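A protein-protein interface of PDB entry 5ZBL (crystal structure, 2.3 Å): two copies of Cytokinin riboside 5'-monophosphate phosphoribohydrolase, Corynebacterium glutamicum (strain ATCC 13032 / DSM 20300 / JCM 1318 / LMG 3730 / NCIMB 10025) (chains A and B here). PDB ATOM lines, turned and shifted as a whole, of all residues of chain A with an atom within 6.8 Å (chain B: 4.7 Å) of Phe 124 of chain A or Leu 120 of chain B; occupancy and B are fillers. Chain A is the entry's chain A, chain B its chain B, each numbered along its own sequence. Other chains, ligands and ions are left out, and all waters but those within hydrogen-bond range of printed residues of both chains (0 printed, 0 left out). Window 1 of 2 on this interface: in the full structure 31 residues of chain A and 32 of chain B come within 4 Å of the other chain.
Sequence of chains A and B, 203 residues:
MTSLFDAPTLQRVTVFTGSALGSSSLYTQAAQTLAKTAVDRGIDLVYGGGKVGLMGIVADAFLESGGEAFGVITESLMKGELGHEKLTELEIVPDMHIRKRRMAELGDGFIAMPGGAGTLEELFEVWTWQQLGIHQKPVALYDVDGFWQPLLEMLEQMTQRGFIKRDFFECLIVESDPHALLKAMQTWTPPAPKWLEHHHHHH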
ATOM      1  N   PHE A  16     -21.492   9.350 -28.630  1.00  0.00           N
ATOM      2  CA  PHE A  16     -22.028   8.066 -29.114  1.00  0.00           C
ATOM      3  C   PHE A  16     -23.044   7.591 -28.081  1.00  0.00           C
ATOM      4  O   PHE A  16     -22.701   7.524 -26.873  1.00  0.00           O
ATOM      5  CB  PHE A  16     -20.924   7.004 -29.214  1.00  0.00           C
ATOM      6  CG  PHE A  16     -19.712   7.420 -30.006  1.00  0.00           C
ATOM      7  CD1 PHE A  16     -19.832   8.084 -31.218  1.00  0.00           C
ATOM      8  CD2 PHE A  16     -18.440   7.049 -29.583  1.00  0.00           C
ATOM      9  CE1 PHE A  16     -18.706   8.441 -31.955  1.00  0.00           C
ATOM     10  CE2 PHE A  16     -17.307   7.374 -30.346  1.00  0.00           C
ATOM     11  CZ  PHE A  16     -17.439   8.079 -31.517  1.00  0.00           C
ATOM     12  N   THR A 119     -23.016   1.829 -30.576  1.00  0.00           N
ATOM     13  CA  THR A 119     -22.300   2.722 -29.688  1.00  0.00           C
ATOM     14  C   THR A 119     -20.933   2.126 -29.338  1.00  0.00           C
ATOM     15  O   THR A 119     -19.914   2.804 -29.376  1.00  0.00           O
ATOM     16  CB  THR A 119     -23.184   3.061 -28.429  1.00  0.00           C
ATOM     17  OG1 THR A 119     -24.381   3.754 -28.857  1.00  0.00           O
ATOM     18  CG2 THR A 119     -22.404   3.909 -27.413  1.00  0.00           C
ATOM     19  N   LEU A 120     -20.942   0.860 -28.987  1.00  0.00           N
ATOM     20  CA  LEU A 120     -19.734   0.119 -28.697  1.00  0.00           C
ATOM     21  C   LEU A 120     -18.776   0.104 -29.881  1.00  0.00           C
ATOM     22  O   LEU A 120     -17.588   0.423 -29.733  1.00  0.00           O
ATOM     23  CB  LEU A 120     -20.079  -1.319 -28.226  1.00  0.00           C
ATOM     24  CG  LEU A 120     -20.150  -1.470 -26.712  1.00  0.00           C
ATOM     25  CD1 LEU A 120     -20.631  -2.825 -26.230  1.00  0.00           C
ATOM     26  CD2 LEU A 120     -18.765  -1.287 -26.146  1.00  0.00           C
ATOM     27  N   GLU A 121     -19.299  -0.219 -31.058  1.00  0.00           N
ATOM     28  CA  GLU A 121     -18.508  -0.152 -32.282  1.00  0.00           C
ATOM     29  C   GLU A 121     -17.831   1.224 -32.487  1.00  0.00           C
ATOM     30  O   GLU A 121     -16.641   1.302 -32.843  1.00  0.00           O
ATOM     31  CB  GLU A 121     -19.370  -0.465 -33.471  1.00  0.00           C
ATOM     32  CG  GLU A 121     -18.638  -0.735 -34.753  1.00  0.00           C
ATOM     33  CD  GLU A 121     -18.225   0.521 -35.487  1.00  0.00           C
ATOM     34  OE1 GLU A 121     -19.011   1.499 -35.472  1.00  0.00           O
ATOM     35  OE2 GLU A 121     -17.101   0.545 -36.086  1.00  0.00           O
ATOM     36  N   GLU A 122     -18.584   2.304 -32.314  1.00  0.00           N
ATOM     37  CA  GLU A 122     -17.997   3.633 -32.514  1.00  0.00           C
ATOM     38  C   GLU A 122     -16.853   3.838 -31.518  1.00  0.00           C
ATOM     39  O   GLU A 122     -15.848   4.412 -31.871  1.00  0.00           O
ATOM     40  CB  GLU A 122     -19.039   4.761 -32.428  1.00  0.00           C
ATOM     41  CG  GLU A 122     -19.762   5.047 -33.748  1.00  0.00           C
ATOM     42  CD  GLU A 122     -21.237   5.466 -33.596  1.00  0.00           C
ATOM     43  OE1 GLU A 122     -21.903   5.040 -32.609  1.00  0.00           O
ATOM     44  OE2 GLU A 122     -21.766   6.194 -34.489  1.00  0.00           O
ATOM     45  N   LEU A 123     -17.007   3.334 -30.299  1.00  0.00           N
ATOM     46  CA  LEU A 123     -16.052   3.578 -29.262  1.00  0.00           C
ATOM     47  C   LEU A 123     -14.729   2.848 -29.564  1.00  0.00           C
ATOM     48  O   LEU A 123     -13.642   3.398 -29.419  1.00  0.00           O
ATOM     49  CB  LEU A 123     -16.632   3.148 -27.910  1.00  0.00           C
ATOM     50  CG  LEU A 123     -15.650   3.227 -26.737  1.00  0.00           C
ATOM     51  CD1 LEU A 123     -15.322   4.651 -26.484  1.00  0.00           C
ATOM     52  CD2 LEU A 123     -16.207   2.555 -25.503  1.00  0.00           C
ATOM     53  N   PHE A 124     -14.846   1.608 -29.988  1.00  0.00           N
ATOM     54  CA  PHE A 124     -13.691   0.805 -30.335  1.00  0.00           C
ATOM     55  C   PHE A 124     -13.007   1.264 -31.617  1.00  0.00           C
ATOM     56  O   PHE A 124     -11.784   1.101 -31.786  1.00  0.00           O
ATOM     57  CB  PHE A 124     -14.084  -0.678 -30.372  1.00  0.00           C
ATOM     58  CG  PHE A 124     -14.102  -1.306 -29.018  1.00  0.00           C
ATOM     59  CD1 PHE A 124     -12.911  -1.499 -28.338  1.00  0.00           C
ATOM     60  CD2 PHE A 124     -15.275  -1.691 -28.413  1.00  0.00           C
ATOM     61  CE1 PHE A 124     -12.887  -2.072 -27.083  1.00  0.00           C
ATOM     62  CE2 PHE A 124     -15.264  -2.252 -27.150  1.00  0.00           C
ATOM     63  CZ  PHE A 124     -14.068  -2.432 -26.486  1.00  0.00           C
ATOM     64  N   GLU A 125     -13.806   1.826 -32.512  1.00  0.00           N
ATOM     65  CA  GLU A 125     -13.321   2.519 -33.687  1.00  0.00           C
ATOM     66  C   GLU A 125     -12.394   3.694 -33.314  1.00  0.00           C
ATOM     67  O   GLU A 125     -11.226   3.739 -33.792  1.00  0.00           O
ATOM     68  CB  GLU A 125     -14.500   2.942 -34.551  1.00  0.00           C
ATOM     69  CG  GLU A 125     -14.222   3.705 -35.834  1.00  0.00           C
ATOM     70  CD  GLU A 125     -13.680   2.853 -36.926  1.00  0.00           C
ATOM     71  OE1 GLU A 125     -14.384   2.613 -37.935  1.00  0.00           O
ATOM     72  OE2 GLU A 125     -12.533   2.441 -36.765  1.00  0.00           O
ATOM     73  N   VAL A 126     -12.820   4.587 -32.418  1.00  0.00           N
ATOM     74  CA  VAL A 126     -11.910   5.704 -32.124  1.00  0.00           C
ATOM     75  C   VAL A 126     -10.644   5.201 -31.422  1.00  0.00           C
ATOM     76  O   VAL A 126      -9.576   5.734 -31.667  1.00  0.00           O
ATOM     77  CB  VAL A 126     -12.553   6.902 -31.398  1.00  0.00           C
ATOM     78  CG1 VAL A 126     -13.802   7.337 -32.135  1.00  0.00           C
ATOM     79  CG2 VAL A 126     -12.865   6.597 -29.955  1.00  0.00           C
ATOM     80  N   TRP A 127     -10.760   4.173 -30.585  1.00  0.00           N
ATOM     81  CA  TRP A 127      -9.581   3.593 -29.935  1.00  0.00           C
ATOM     82  C   TRP A 127      -8.609   2.971 -30.918  1.00  0.00           C
ATOM     83  O   TRP A 127      -7.411   3.208 -30.846  1.00  0.00           O
ATOM     84  CB  TRP A 127      -9.969   2.519 -28.891  1.00  0.00           C
ATOM     85  CG  TRP A 127     -10.306   3.058 -27.562  1.00  0.00           C
ATOM     86  CD1 TRP A 127      -9.868   4.231 -27.001  1.00  0.00           C
ATOM     87  CD2 TRP A 127     -11.131   2.434 -26.585  1.00  0.00           C
ATOM     88  NE1 TRP A 127     -10.383   4.372 -25.752  1.00  0.00           N
ATOM     89  CE2 TRP A 127     -11.166   3.286 -25.466  1.00  0.00           C
ATOM     90  CE3 TRP A 127     -11.855   1.245 -26.550  1.00  0.00           C
ATOM     91  CZ2 TRP A 127     -11.896   2.981 -24.322  1.00  0.00           C
ATOM     92  CZ3 TRP A 127     -12.579   0.941 -25.414  1.00  0.00           C
ATOM     93  CH2 TRP A 127     -12.605   1.809 -24.319  1.00  0.00           C
ATOM     94  N   THR A 128      -9.131   2.143 -31.807  1.00  0.00           N
ATOM     95  CA  THR A 128      -8.337   1.570 -32.869  1.00  0.00           C
ATOM     96  C   THR A 128      -7.602   2.675 -33.637  1.00  0.00           C
ATOM     97  O   THR A 128      -6.489   2.449 -34.089  1.00  0.00           O
ATOM     98  CB  THR A 128      -9.214   0.753 -33.834  1.00  0.00           C
ATOM     99  OG1 THR A 128      -9.929  -0.250 -33.094  1.00  0.00           O
ATOM    100  CG2 THR A 128      -8.379   0.084 -34.905  1.00  0.00           C
ATOM    101  N   TRP A 129      -8.226   3.849 -33.776  1.00  0.00           N
ATOM    102  CA  TRP A 129      -7.589   5.011 -34.408  1.00  0.00           C
ATOM    103  C   TRP A 129      -6.565   5.681 -33.493  1.00  0.00           C
ATOM    104  O   TRP A 129      -5.464   6.007 -33.951  1.00  0.00           O
ATOM    105  CB  TRP A 129      -8.628   6.052 -34.845  1.00  0.00           C
ATOM    106  CG  TRP A 129      -9.431   5.676 -36.006  1.00  0.00           C
ATOM    107  CD1 TRP A 129      -9.158   4.702 -36.918  1.00  0.00           C
ATOM    108  CD2 TRP A 129     -10.665   6.284 -36.423  1.00  0.00           C
ATOM    109  NE1 TRP A 129     -10.152   4.651 -37.866  1.00  0.00           N
ATOM    110  CE2 TRP A 129     -11.093   5.606 -37.587  1.00  0.00           C
ATOM    111  CE3 TRP A 129     -11.459   7.326 -35.918  1.00  0.00           C
ATOM    112  CZ2 TRP A 129     -12.289   5.933 -38.261  1.00  0.00           C
ATOM    113  CZ3 TRP A 129     -12.659   7.649 -36.591  1.00  0.00           C
ATOM    114  CH2 TRP A 129     -13.049   6.960 -37.751  1.00  0.00           C
ATOM    115  N   TRP A 148     -20.528   1.147 -17.796  1.00  0.00           N
ATOM    116  CA  TRP A 148     -19.325   0.734 -18.456  1.00  0.00           C
ATOM    117  C   TRP A 148     -18.465  -0.205 -17.612  1.00  0.00           C
ATOM    118  O   TRP A 148     -17.480  -0.704 -18.098  1.00  0.00           O
ATOM    119  CB  TRP A 148     -18.532   1.941 -18.931  1.00  0.00           C
ATOM    120  CG  TRP A 148     -19.218   2.677 -19.951  1.00  0.00           C
ATOM    121  CD1 TRP A 148     -19.786   3.894 -19.822  1.00  0.00           C
ATOM    122  CD2 TRP A 148     -19.418   2.271 -21.297  1.00  0.00           C
ATOM    123  NE1 TRP A 148     -20.331   4.285 -21.004  1.00  0.00           N
ATOM    124  CE2 TRP A 148     -20.130   3.305 -21.936  1.00  0.00           C
ATOM    125  CE3 TRP A 148     -19.035   1.144 -22.043  1.00  0.00           C
ATOM    126  CZ2 TRP A 148     -20.489   3.254 -23.290  1.00  0.00           C
ATOM    127  CZ3 TRP A 148     -19.396   1.076 -23.397  1.00  0.00           C
ATOM    128  CH2 TRP A 148     -20.115   2.147 -24.010  1.00  0.00           C
ATOM    129  N   LEU A 151     -17.318  -3.636 -19.291  1.00  0.00           N
ATOM    130  CA  LEU A 151     -16.369  -3.453 -20.383  1.00  0.00           C
ATOM    131  C   LEU A 151     -14.987  -3.154 -19.860  1.00  0.00           C
ATOM    132  O   LEU A 151     -14.004  -3.572 -20.452  1.00  0.00           O
ATOM    133  CB  LEU A 151     -16.784  -2.304 -21.288  1.00  0.00           C
ATOM    134  CG  LEU A 151     -15.905  -2.188 -22.529  1.00  0.00           C
ATOM    135  CD1 LEU A 151     -16.285  -3.204 -23.606  1.00  0.00           C
ATOM    136  CD2 LEU A 151     -15.961  -0.760 -23.016  1.00  0.00           C
ATOM    137  N   MET A 154     -13.459  -6.311 -19.002  1.00  0.00           N
ATOM    138  CA  MET A 154     -13.023  -6.940 -20.220  1.00  0.00           C
ATOM    139  C   MET A 154     -11.675  -6.387 -20.665  1.00  0.00           C
ATOM    140  O   MET A 154     -10.813  -7.178 -20.998  1.00  0.00           O
ATOM    141  CB  MET A 154     -14.077  -6.818 -21.353  1.00  0.00           C
ATOM    142  CG  MET A 154     -13.732  -7.549 -22.677  1.00  0.00           C
ATOM    143  SD  MET A 154     -13.462  -9.363 -22.595  1.00  0.00           S
ATOM    144  CE  MET A 154     -12.657  -9.680 -24.153  1.00  0.00           C
ATOM    145  N   LEU A 155     -11.525  -5.059 -20.673  1.00  0.00           N
ATOM    146  CA  LEU A 155     -10.322  -4.398 -21.105  1.00  0.00           C
ATOM    147  C   LEU A 155      -9.149  -4.638 -20.182  1.00  0.00           C
ATOM    148  O   LEU A 155      -8.027  -4.752 -20.634  1.00  0.00           O
ATOM    149  CB  LEU A 155     -10.524  -2.883 -21.191  1.00  0.00           C
ATOM    150  CG  LEU A 155     -11.436  -2.402 -22.307  1.00  0.00           C
ATOM    151  CD1 LEU A 155     -11.476  -0.873 -22.269  1.00  0.00           C
ATOM    152  CD2 LEU A 155     -10.971  -2.892 -23.673  1.00  0.00           C
ATOM    153  N   MET A 158      -8.092  -8.145 -21.108  1.00  0.00           N
ATOM    154  CA  MET A 158      -7.356  -8.098 -22.348  1.00  0.00           C
ATOM    155  C   MET A 158      -5.919  -7.554 -22.152  1.00  0.00           C
ATOM    156  O   MET A 158      -5.014  -7.990 -22.842  1.00  0.00           O
ATOM    157  CB  MET A 158      -8.094  -7.238 -23.349  1.00  0.00           C
ATOM    158  CG  MET A 158      -9.392  -7.810 -23.864  1.00  0.00           C
ATOM    159  SD  MET A 158     -10.256  -6.619 -24.935  1.00  0.00           S
ATOM    160  CE  MET A 158     -10.800  -7.771 -26.174  1.00  0.00           C
ATOM    161  N   ILE A 164      -3.695  -5.725 -25.342  1.00  0.00           N
ATOM    162  CA  ILE A 164      -3.681  -4.263 -25.286  1.00  0.00           C
ATOM    163  C   ILE A 164      -2.522  -3.813 -24.380  1.00  0.00           C
ATOM    164  O   ILE A 164      -2.180  -4.493 -23.424  1.00  0.00           O
ATOM    165  CB  ILE A 164      -4.998  -3.722 -24.674  1.00  0.00           C
ATOM    166  CG1 ILE A 164      -6.204  -4.259 -25.453  1.00  0.00           C
ATOM    167  CG2 ILE A 164      -4.992  -2.191 -24.647  1.00  0.00           C
ATOM    168  CD1 ILE A 164      -7.520  -3.992 -24.787  1.00  0.00           C
ATOM    169  N   GLY B 116      -7.287  -7.586 -29.422  1.00  0.00           N
ATOM    170  CA  GLY B 116      -7.421  -6.275 -28.761  1.00  0.00           C
ATOM    171  C   GLY B 116      -8.543  -5.427 -29.349  1.00  0.00           C
ATOM    172  O   GLY B 116      -9.600  -5.943 -29.780  1.00  0.00           O
ATOM    173  N   ALA B 117      -8.306  -4.120 -29.376  1.00  0.00           N
ATOM    174  CA  ALA B 117      -9.349  -3.146 -29.756  1.00  0.00           C
ATOM    175  C   ALA B 117      -9.934  -3.432 -31.131  1.00  0.00           C
ATOM    176  O   ALA B 117     -11.131  -3.269 -31.346  1.00  0.00           O
ATOM    177  CB  ALA B 117      -8.787  -1.730 -29.743  1.00  0.00           C
ATOM    178  N   GLY B 118      -9.050  -3.832 -32.055  1.00  0.00           N
ATOM    179  CA  GLY B 118      -9.381  -4.070 -33.467  1.00  0.00           C
ATOM    180  C   GLY B 118     -10.364  -5.216 -33.657  1.00  0.00           C
ATOM    181  O   GLY B 118     -11.320  -5.116 -34.416  1.00  0.00           O
ATOM    182  N   THR B 119     -10.109  -6.299 -32.943  1.00  0.00           N
ATOM    183  CA  THR B 119     -10.942  -7.469 -32.999  1.00  0.00           C
ATOM    184  C   THR B 119     -12.295  -7.124 -32.489  1.00  0.00           C
ATOM    185  O   THR B 119     -13.268  -7.528 -33.080  1.00  0.00           O
ATOM    186  CB  THR B 119     -10.324  -8.611 -32.160  1.00  0.00           C
ATOM    187  OG1 THR B 119      -9.090  -8.984 -32.756  1.00  0.00           O
ATOM    188  CG2 THR B 119     -11.222  -9.820 -32.114  1.00  0.00           C
ATOM    189  N   LEU B 120     -12.360  -6.356 -31.403  1.00  0.00           N
ATOM    190  CA  LEU B 120     -13.648  -5.969 -30.800  1.00  0.00           C
ATOM    191  C   LEU B 120     -14.438  -5.069 -31.719  1.00  0.00           C
ATOM    192  O   LEU B 120     -15.683  -5.230 -31.839  1.00  0.00           O
ATOM    193  CB  LEU B 120     -13.471  -5.327 -29.438  1.00  0.00           C
ATOM    194  CG  LEU B 120     -13.206  -6.230 -28.232  1.00  0.00           C
ATOM    195  CD1 LEU B 120     -13.084  -5.391 -26.973  1.00  0.00           C
ATOM    196  CD2 LEU B 120     -14.348  -7.202 -28.075  1.00  0.00           C
ATOM    197  N   GLU B 121     -13.711  -4.180 -32.405  1.00  0.00           N
ATOM    198  CA  GLU B 121     -14.311  -3.252 -33.340  1.00  0.00           C
ATOM    199  C   GLU B 121     -14.955  -4.021 -34.438  1.00  0.00           C
ATOM    200  O   GLU B 121     -16.143  -3.790 -34.714  1.00  0.00           O
ATOM    201  CB  GLU B 121     -13.323  -2.220 -33.889  1.00  0.00           C
ATOM    202  CG  GLU B 121     -13.937  -1.180 -34.844  1.00  0.00           C
ATOM    203  CD  GLU B 121     -14.359  -1.769 -36.198  1.00  0.00           C
ATOM    204  OE1 GLU B 121     -13.646  -2.655 -36.718  1.00  0.00           O
ATOM    205  OE2 GLU B 121     -15.413  -1.367 -36.747  1.00  0.00           O
ATOM    206  N   GLU B 122     -14.191  -4.936 -35.047  1.00  0.00           N
ATOM    207  CA  GLU B 122     -14.718  -5.802 -36.123  1.00  0.00           C
ATOM    208  C   GLU B 122     -15.958  -6.514 -35.645  1.00  0.00           C
ATOM    209  O   GLU B 122     -16.985  -6.485 -36.263  1.00  0.00           O
ATOM    210  CB  GLU B 122     -13.650  -6.792 -36.649  1.00  0.00           C
ATOM    211  CG  GLU B 122     -12.609  -6.080 -37.510  1.00  0.00           C
ATOM    212  CD  GLU B 122     -11.345  -6.877 -37.881  1.00  0.00           C
ATOM    213  OE1 GLU B 122     -10.758  -7.602 -37.033  1.00  0.00           O
ATOM    214  OE2 GLU B 122     -10.917  -6.740 -39.057  1.00  0.00           O
ATOM    215  N   LEU B 123     -15.880  -7.087 -34.472  1.00  0.00           N
ATOM    216  CA  LEU B 123     -17.004  -7.850 -33.963  1.00  0.00           C
ATOM    217  C   LEU B 123     -18.253  -6.979 -33.732  1.00  0.00           C
ATOM    218  O   LEU B 123     -19.388  -7.344 -34.113  1.00  0.00           O
ATOM    219  CB  LEU B 123     -16.545  -8.520 -32.680  1.00  0.00           C
ATOM    220  CG  LEU B 123     -17.476  -9.445 -31.998  1.00  0.00           C
ATOM    221  CD1 LEU B 123     -17.886 -10.569 -32.915  1.00  0.00           C
ATOM    222  CD2 LEU B 123     -16.730  -9.952 -30.786  1.00  0.00           C
ATOM    223  N   PHE B 124     -18.046  -5.815 -33.144  1.00  0.00           N
ATOM    224  CA  PHE B 124     -19.164  -4.901 -32.969  1.00  0.00           C
ATOM    225  C   PHE B 124     -19.754  -4.389 -34.273  1.00  0.00           C
ATOM    226  O   PHE B 124     -20.984  -4.243 -34.382  1.00  0.00           O
ATOM    227  CB  PHE B 124     -18.817  -3.788 -31.990  1.00  0.00           C
ATOM    228  CG  PHE B 124     -18.887  -4.246 -30.586  1.00  0.00           C
ATOM    229  CD1 PHE B 124     -20.124  -4.456 -29.995  1.00  0.00           C
ATOM    230  CD2 PHE B 124     -17.748  -4.585 -29.892  1.00  0.00           C
ATOM    231  CE1 PHE B 124     -20.216  -4.916 -28.704  1.00  0.00           C
ATOM    232  CE2 PHE B 124     -17.824  -5.077 -28.612  1.00  0.00           C
ATOM    233  CZ  PHE B 124     -19.059  -5.254 -28.029  1.00  0.00           C
ATOM    234  N   TRP B 148     -13.794 -14.708 -23.724  1.00  0.00           N
ATOM    235  CA  TRP B 148     -14.939 -13.870 -24.065  1.00  0.00           C
ATOM    236  C   TRP B 148     -15.907 -13.659 -22.902  1.00  0.00           C
ATOM    237  O   TRP B 148     -16.838 -12.903 -23.046  1.00  0.00           O
ATOM    238  CB  TRP B 148     -15.662 -14.402 -25.311  1.00  0.00           C
ATOM    239  CG  TRP B 148     -14.882 -14.246 -26.526  1.00  0.00           C
ATOM    240  CD1 TRP B 148     -14.360 -15.240 -27.297  1.00  0.00           C
ATOM    241  CD2 TRP B 148     -14.487 -13.021 -27.122  1.00  0.00           C
ATOM    242  NE1 TRP B 148     -13.677 -14.700 -28.348  1.00  0.00           N
ATOM    243  CE2 TRP B 148     -13.744 -13.340 -28.273  1.00  0.00           C
ATOM    244  CE3 TRP B 148     -14.724 -11.668 -26.811  1.00  0.00           C
ATOM    245  CZ2 TRP B 148     -13.214 -12.370 -29.118  1.00  0.00           C
ATOM    246  CZ3 TRP B 148     -14.185 -10.704 -27.619  1.00  0.00           C
ATOM    247  CH2 TRP B 148     -13.427 -11.059 -28.780  1.00  0.00           C
ATOM    248  N   LEU B 151     -16.920 -10.013 -21.762  1.00  0.00           N
ATOM    249  CA  LEU B 151     -17.794  -9.499 -22.801  1.00  0.00           C
ATOM    250  C   LEU B 151     -19.249  -9.989 -22.736  1.00  0.00           C
ATOM    251  O   LEU B 151     -20.173  -9.194 -22.948  1.00  0.00           O
ATOM    252  CB  LEU B 151     -17.244  -9.816 -24.193  1.00  0.00           C
ATOM    253  CG  LEU B 151     -17.995  -9.074 -25.312  1.00  0.00           C
ATOM    254  CD1 LEU B 151     -17.704  -7.573 -25.285  1.00  0.00           C
ATOM    255  CD2 LEU B 151     -17.713  -9.639 -26.673  1.00  0.00           C
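Of the 11 printed residues of chain B, 7 touch a printed residue of chain A. Hydrophobic or aromatic side chains of chain B that line the printed part of chain A: Ala 117, Leu 120, Phe 124 and Trp 148.
N of Leu 151 of chain B is in hydrogen-bond range of SD of Met 154 of chain A (3.6 Å). The side-chain carboxylate of Glu 121 of chain B sits close to the side-chain carboxylate of Glu 121 of chain A.
Phe 124 of chain A touches just these residues of chain B: Ala 117, Leu 120 and Glu 121. Leu 120 of chain B touches just these residues of chain A: Phe 124 (3.2 Å) and Met 158 (3.4 Å). Printed residues of chain A within 4 Å of Phe 124 of chain B: Leu 120 and Glu 121. Printed residues of chain B within 4 Å of Met 154 of chain A: Trp 148 and Leu 151. Of the printed residues of chain B, Thr 128 of chain A touches Ala 117 (3.7 Å) and Gly 118 (3.8 Å). Thr 119 of chain B touches none of the printed residues of chain A. Phe 16 of chain A touches none of the printed residues of chain B. The nearest residue of chain A that does not touch Leu 120 of chain B is Leu 155 of chain A (4.6 Å).
OG1 of Thr 128 of chain A lies within hydrogen-bond range of O of Phe 124 of chain A, at 2.6 Å. The side-chain carboxylate (OE2) of Glu 125 of chain A lies within hydrogen-bond range of the indole nitrogen (NE1) of Trp 129 of chain A (3.4 Å).
CE1 of Phe 124 of chain B touches CD1 of Leu 120 of chain A, at 3.3 Å. Glu 121 of chain A touches Phe 124 of chain B (CA to CB, 3.7 Å). Phe 124 of chain A touches Ala 117 of chain B. Leu 120 of chain B touches Phe 124 of chain A (CD1 to CZ, 3.2 Å). CB of Phe 124 of chain A touches CB of Glu 121 of chain B (3.9 Å). Glu 125 of chain A touches Glu 121 of chain B. Thr 128 of chain A touches Ala 117 of chain B (OG1 to O, 3.7 Å). OG1 of Thr 128 of chain A touches N of Gly 118 of chain B, at 3.8 Å. Trp 148 of chain B touches Met 154 of chain A. CE of Met 158 of chain A touches CD1 of Leu 120 of chain B (3.4 Å).
Leu 120 of chain A touches Phe 124 of chain B, and with the chains exchanged Phe 124 of chain A touches Leu 120 of chain B. Glu 121 of chain B touches its own counterpart, Glu 121 of chain A. Glu 121 of chain A touches Phe 124 of chain B, and with the chains exchanged Phe 124 of chain A touches Glu 121 of chain B. Positions printed for both chains: 119, 120, 121, 122, 123, 124, 148 and 151. Of the 12 pairs that touch across the chains among the printed residues, 5 have their exchanged pair printed and touching as well.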
